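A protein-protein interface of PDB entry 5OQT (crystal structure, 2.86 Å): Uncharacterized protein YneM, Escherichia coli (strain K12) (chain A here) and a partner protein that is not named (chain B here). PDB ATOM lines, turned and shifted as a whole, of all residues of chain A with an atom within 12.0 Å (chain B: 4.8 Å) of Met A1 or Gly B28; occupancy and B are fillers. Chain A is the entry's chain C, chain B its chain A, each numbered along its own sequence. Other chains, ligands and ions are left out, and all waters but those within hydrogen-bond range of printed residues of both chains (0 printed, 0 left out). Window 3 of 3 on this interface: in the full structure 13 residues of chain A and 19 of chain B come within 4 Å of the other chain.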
ATOM      1  N   MET A   1      -0.009 -11.595   1.152  1.00  0.00           N
ATOM      2  CA  MET A   1       0.319 -11.724   2.567  1.00  0.00           C
ATOM      3  C   MET A   1       1.115 -10.499   3.010  1.00  0.00           C
ATOM      4  O   MET A   1       1.315  -9.598   2.187  1.00  0.00           O
ATOM      5  CB  MET A   1       1.072 -13.040   2.837  1.00  0.00           C
ATOM      6  CG  MET A   1       0.544 -13.780   4.040  1.00  0.00           C
ATOM      7  SD  MET A   1       0.781 -15.568   3.961  1.00  0.00           S
ATOM      8  CE  MET A   1       1.946 -15.819   5.293  1.00  0.00           C
ATOM      9  N   LEU A   2       1.548 -10.454   4.303  1.00  0.00           N
ATOM     10  CA  LEU A   2       2.276  -9.351   4.964  1.00  0.00           C
ATOM     11  C   LEU A   2       1.358  -8.138   5.109  1.00  0.00           C
ATOM     12  O   LEU A   2       1.041  -7.760   6.233  1.00  0.00           O
ATOM     13  CB  LEU A   2       3.654  -9.006   4.316  1.00  0.00           C
ATOM     14  CG  LEU A   2       4.642  -8.048   5.059  1.00  0.00           C
ATOM     15  CD1 LEU A   2       4.400  -6.569   4.719  1.00  0.00           C
ATOM     16  CD2 LEU A   2       4.721  -8.317   6.570  1.00  0.00           C
ATOM     17  N   GLY A   3       0.921  -7.576   3.979  1.00  0.00           N
ATOM     18  CA  GLY A   3      -0.031  -6.475   3.922  1.00  0.00           C
ATOM     19  C   GLY A   3      -1.344  -6.909   4.534  1.00  0.00           C
ATOM     20  O   GLY A   3      -1.951  -6.158   5.298  1.00  0.00           O
ATOM     21  N   ASN A   4      -1.739  -8.166   4.268  1.00  0.00           N
ATOM     22  CA  ASN A   4      -2.943  -8.786   4.818  1.00  0.00           C
ATOM     23  C   ASN A   4      -2.845  -9.001   6.332  1.00  0.00           C
ATOM     24  O   ASN A   4      -3.860  -8.870   7.014  1.00  0.00           O
ATOM     25  CB  ASN A   4      -3.291 -10.064   4.065  1.00  0.00           C
ATOM     26  CG  ASN A   4      -3.671  -9.826   2.618  1.00  0.00           C
ATOM     27  OD1 ASN A   4      -3.765  -8.688   2.138  1.00  0.00           O
ATOM     28  ND2 ASN A   4      -3.908 -10.903   1.886  1.00  0.00           N
ATOM     29  N   MET A   5      -1.624  -9.275   6.853  1.00  0.00           N
ATOM     30  CA  MET A   5      -1.334  -9.419   8.286  1.00  0.00           C
ATOM     31  C   MET A   5      -1.458  -8.053   8.979  1.00  0.00           C
ATOM     32  O   MET A   5      -2.108  -7.948  10.020  1.00  0.00           O
ATOM     33  CB  MET A   5       0.086  -9.954   8.492  1.00  0.00           C
ATOM     34  CG  MET A   5       0.149 -11.412   8.844  1.00  0.00           C
ATOM     35  SD  MET A   5       1.818 -12.106   8.665  1.00  0.00           S
ATOM     36  CE  MET A   5       1.837 -12.424   6.975  1.00  0.00           C
ATOM     37  N   ASN A   6      -0.833  -7.010   8.388  1.00  0.00           N
ATOM     38  CA  ASN A   6      -0.835  -5.635   8.884  1.00  0.00           C
ATOM     39  C   ASN A   6      -2.244  -5.071   8.867  1.00  0.00           C
ATOM     40  O   ASN A   6      -2.640  -4.452   9.852  1.00  0.00           O
ATOM     41  CB  ASN A   6       0.121  -4.744   8.068  1.00  0.00           C
ATOM     42  CG  ASN A   6       1.574  -5.175   8.060  1.00  0.00           C
ATOM     43  OD1 ASN A   6       2.074  -5.836   8.984  1.00  0.00           O
ATOM     44  ND2 ASN A   6       2.290  -4.800   6.998  1.00  0.00           N
ATOM     45  N   VAL A   7      -3.006  -5.312   7.770  1.00  0.00           N
ATOM     46  CA  VAL A   7      -4.400  -4.876   7.589  1.00  0.00           C
ATOM     47  C   VAL A   7      -5.287  -5.487   8.692  1.00  0.00           C
ATOM     48  O   VAL A   7      -6.067  -4.762   9.316  1.00  0.00           O
ATOM     49  CB  VAL A   7      -4.910  -5.135   6.138  1.00  0.00           C
ATOM     50  CG1 VAL A   7      -6.417  -5.355   6.071  1.00  0.00           C
ATOM     51  CG2 VAL A   7      -4.501  -4.002   5.209  1.00  0.00           C
ATOM     52  N   PHE A   8      -5.105  -6.792   8.973  1.00  0.00           N
ATOM     53  CA  PHE A   8      -5.817  -7.514  10.025  1.00  0.00           C
ATOM     54  C   PHE A   8      -5.528  -6.878  11.405  1.00  0.00           C
ATOM     55  O   PHE A   8      -6.457  -6.462  12.106  1.00  0.00           O
ATOM     56  CB  PHE A   8      -5.418  -9.009  10.002  1.00  0.00           C
ATOM     57  CG  PHE A   8      -5.884  -9.842  11.177  1.00  0.00           C
ATOM     58  CD1 PHE A   8      -7.185 -10.329  11.232  1.00  0.00           C
ATOM     59  CD2 PHE A   8      -5.011 -10.172  12.208  1.00  0.00           C
ATOM     60  CE1 PHE A   8      -7.616 -11.091  12.316  1.00  0.00           C
ATOM     61  CE2 PHE A   8      -5.444 -10.938  13.293  1.00  0.00           C
ATOM     62  CZ  PHE A   8      -6.744 -11.383  13.343  1.00  0.00           C
ATOM     63  N   MET A   9      -4.233  -6.790  11.765  1.00  0.00           N
ATOM     64  CA  MET A   9      -3.744  -6.231  13.022  1.00  0.00           C
ATOM     65  C   MET A   9      -4.219  -4.808  13.286  1.00  0.00           C
ATOM     66  O   MET A   9      -4.606  -4.499  14.413  1.00  0.00           O
ATOM     67  CB  MET A   9      -2.216  -6.304  13.064  1.00  0.00           C
ATOM     68  CG  MET A   9      -1.701  -7.619  13.552  1.00  0.00           C
ATOM     69  SD  MET A   9      -2.089  -7.821  15.301  1.00  0.00           S
ATOM     70  CE  MET A   9      -0.437  -8.126  15.958  1.00  0.00           C
ATOM     71  N   GLU B  26      -0.499 -16.669  -4.380  1.00  0.00           N
ATOM     72  CA  GLU B  26       0.072 -15.732  -3.411  1.00  0.00           C
ATOM     73  C   GLU B  26      -0.197 -16.254  -1.994  1.00  0.00           C
ATOM     74  O   GLU B  26       0.680 -16.173  -1.123  1.00  0.00           O
ATOM     75  CB  GLU B  26      -0.557 -14.326  -3.606  1.00  0.00           C
ATOM     76  CG  GLU B  26      -0.255 -13.270  -2.532  1.00  0.00           C
ATOM     77  CD  GLU B  26      -1.244 -13.144  -1.378  1.00  0.00           C
ATOM     78  OE1 GLU B  26      -0.984 -13.743  -0.308  1.00  0.00           O
ATOM     79  OE2 GLU B  26      -2.248 -12.407  -1.519  1.00  0.00           O
ATOM     80  N   LEU B  27      -1.437 -16.735  -1.771  1.00  0.00           N
ATOM     81  CA  LEU B  27      -1.973 -17.225  -0.507  1.00  0.00           C
ATOM     82  C   LEU B  27      -1.019 -18.132   0.263  1.00  0.00           C
ATOM     83  O   LEU B  27      -0.443 -19.068  -0.302  1.00  0.00           O
ATOM     84  CB  LEU B  27      -3.340 -17.906  -0.727  1.00  0.00           C
ATOM     85  CG  LEU B  27      -4.550 -16.969  -0.876  1.00  0.00           C
ATOM     86  CD1 LEU B  27      -4.740 -16.513  -2.308  1.00  0.00           C
ATOM     87  CD2 LEU B  27      -5.818 -17.650  -0.427  1.00  0.00           C
ATOM     88  N   GLY B  28      -0.825 -17.789   1.533  1.00  0.00           N
ATOM     89  CA  GLY B  28       0.016 -18.528   2.465  1.00  0.00           C
ATOM     90  C   GLY B  28      -0.763 -19.001   3.677  1.00  0.00           C
ATOM     91  O   GLY B  28      -2.000 -18.997   3.661  1.00  0.00           O
ATOM     92  N   ALA B  29      -0.039 -19.411   4.741  1.00  0.00           N
ATOM     93  CA  ALA B  29      -0.614 -19.918   5.990  1.00  0.00           C
ATOM     94  C   ALA B  29      -1.512 -18.910   6.700  1.00  0.00           C
ATOM     95  O   ALA B  29      -2.498 -19.328   7.303  1.00  0.00           O
ATOM     96  CB  ALA B  29       0.481 -20.398   6.925  1.00  0.00           C
ATOM     97  N   PHE B  30      -1.200 -17.599   6.623  1.00  0.00           N
ATOM     98  CA  PHE B  30      -2.016 -16.567   7.262  1.00  0.00           C
ATOM     99  C   PHE B  30      -3.372 -16.401   6.558  1.00  0.00           C
ATOM    100  O   PHE B  30      -4.415 -16.373   7.234  1.00  0.00           O
ATOM    101  CB  PHE B  30      -1.274 -15.213   7.346  1.00  0.00           C
ATOM    102  CG  PHE B  30      -2.139 -14.086   7.877  1.00  0.00           C
ATOM    103  CD1 PHE B  30      -2.757 -13.192   7.007  1.00  0.00           C
ATOM    104  CD2 PHE B  30      -2.392 -13.963   9.243  1.00  0.00           C
ATOM    105  CE1 PHE B  30      -3.599 -12.188   7.497  1.00  0.00           C
ATOM    106  CE2 PHE B  30      -3.214 -12.940   9.733  1.00  0.00           C
ATOM    107  CZ  PHE B  30      -3.821 -12.069   8.857  1.00  0.00           C
ATOM    108  N   ASP B  31      -3.342 -16.267   5.206  1.00  0.00           N
ATOM    109  CA  ASP B  31      -4.515 -16.065   4.351  1.00  0.00           C
ATOM    110  C   ASP B  31      -5.508 -17.198   4.467  1.00  0.00           C
ATOM    111  O   ASP B  31      -6.715 -16.971   4.356  1.00  0.00           O
ATOM    112  CB  ASP B  31      -4.094 -15.882   2.890  1.00  0.00           C
ATOM    113  CG  ASP B  31      -3.247 -14.653   2.642  1.00  0.00           C
ATOM    114  OD1 ASP B  31      -2.073 -14.814   2.238  1.00  0.00           O
ATOM    115  OD2 ASP B  31      -3.757 -13.528   2.846  1.00  0.00           O
ATOM    116  N   LEU B  32      -4.996 -18.416   4.692  1.00  0.00           N
ATOM    117  CA  LEU B  32      -5.796 -19.624   4.857  1.00  0.00           C
ATOM    118  C   LEU B  32      -6.370 -19.732   6.269  1.00  0.00           C
ATOM    119  O   LEU B  32      -7.450 -20.295   6.420  1.00  0.00           O
ATOM    120  CB  LEU B  32      -5.006 -20.882   4.455  1.00  0.00           C
ATOM    121  CG  LEU B  32      -4.599 -21.003   2.970  1.00  0.00           C
ATOM    122  CD1 LEU B  32      -3.430 -21.932   2.817  1.00  0.00           C
ATOM    123  CD2 LEU B  32      -5.753 -21.474   2.094  1.00  0.00           C
ATOM    124  N   ASP B 252       0.698 -25.562   3.719  1.00  0.00           N
ATOM    125  CA  ASP B 252      -0.008 -24.364   4.176  1.00  0.00           C
ATOM    126  C   ASP B 252      -1.466 -24.649   4.541  1.00  0.00           C
ATOM    127  O   ASP B 252      -1.929 -24.159   5.575  1.00  0.00           O
ATOM    128  CB  ASP B 252       0.133 -23.203   3.185  1.00  0.00           C
ATOM    129  CG  ASP B 252       1.511 -22.553   3.191  1.00  0.00           C
ATOM    130  OD1 ASP B 252       2.228 -22.675   4.221  1.00  0.00           O
ATOM    131  OD2 ASP B 252       1.866 -21.900   2.173  1.00  0.00           O
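The backbone NH of Gly B28 sits at hydrogen-bond distance from the side-chain carboxylate of Asp B31 (3.3 Å).
Of the 8 printed residues of chain B, 4 touch a printed residue of chain A.
Hydrophobic or aromatic side chains of chain B that line the printed part of chain A: Phe B30.
Of the 9 printed residues of chain A, 4 touch a printed residue of chain B.
Printed residues of chain A that touch a printed residue of chain B: Met A1, Asn A4, Met A5 and Phe A8.
Hydrophobic or aromatic side chains of chain A within 4 Å of the printed part of chain B: Met A1, Met A5 and Phe A8.
Along chain A the printed residues that touch a printed residue of chain B span positions 1 to 8.
Of chain A, only Met A1 (3.4 Å) comes within 4 Å of Gly B28.
Glu B26 touches one residue of chain A.
Phe B30 touches four residues of chain A.
Asp B31 touches two residues of chain A.
No residue of chain A comes within 4 Å of Leu B32.
No residue of chain A comes within 4 Å of Asp B252.
Of the printed residues of chain B, Asn A4 touches Phe B30 and Asp B31.
Printed residues of chain B within 4 Å of Met A5: Phe B30 (3.6 Å).
Leu A2 touches none of the printed residues of chain B.
CE of Met A1 touches N of Phe B30, 3.9 Å away.
Phe B30 touches Asn A4 (CE1 to O, 3.4 Å).
Met A5 touches Phe B30 (N to CE1, 3.6 Å).
Phe B30 touches Phe A8 (CZ to CB, 3.6 Å).
The backbone NH of Gly B28 sits close to the side-chain sulfur of Met A1, 3.7 Å away.
OE1 of Glu B26 is in hydrogen-bond range of N of Met A1.
The side-chain carboxylate of Asp B31 lies close to the side-chain sulfur of Met A1, 3.4 Å away.
OD2 of Asp B31 sits at hydrogen-bond distance from ND2 of Asn A4 (2.8 Å).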
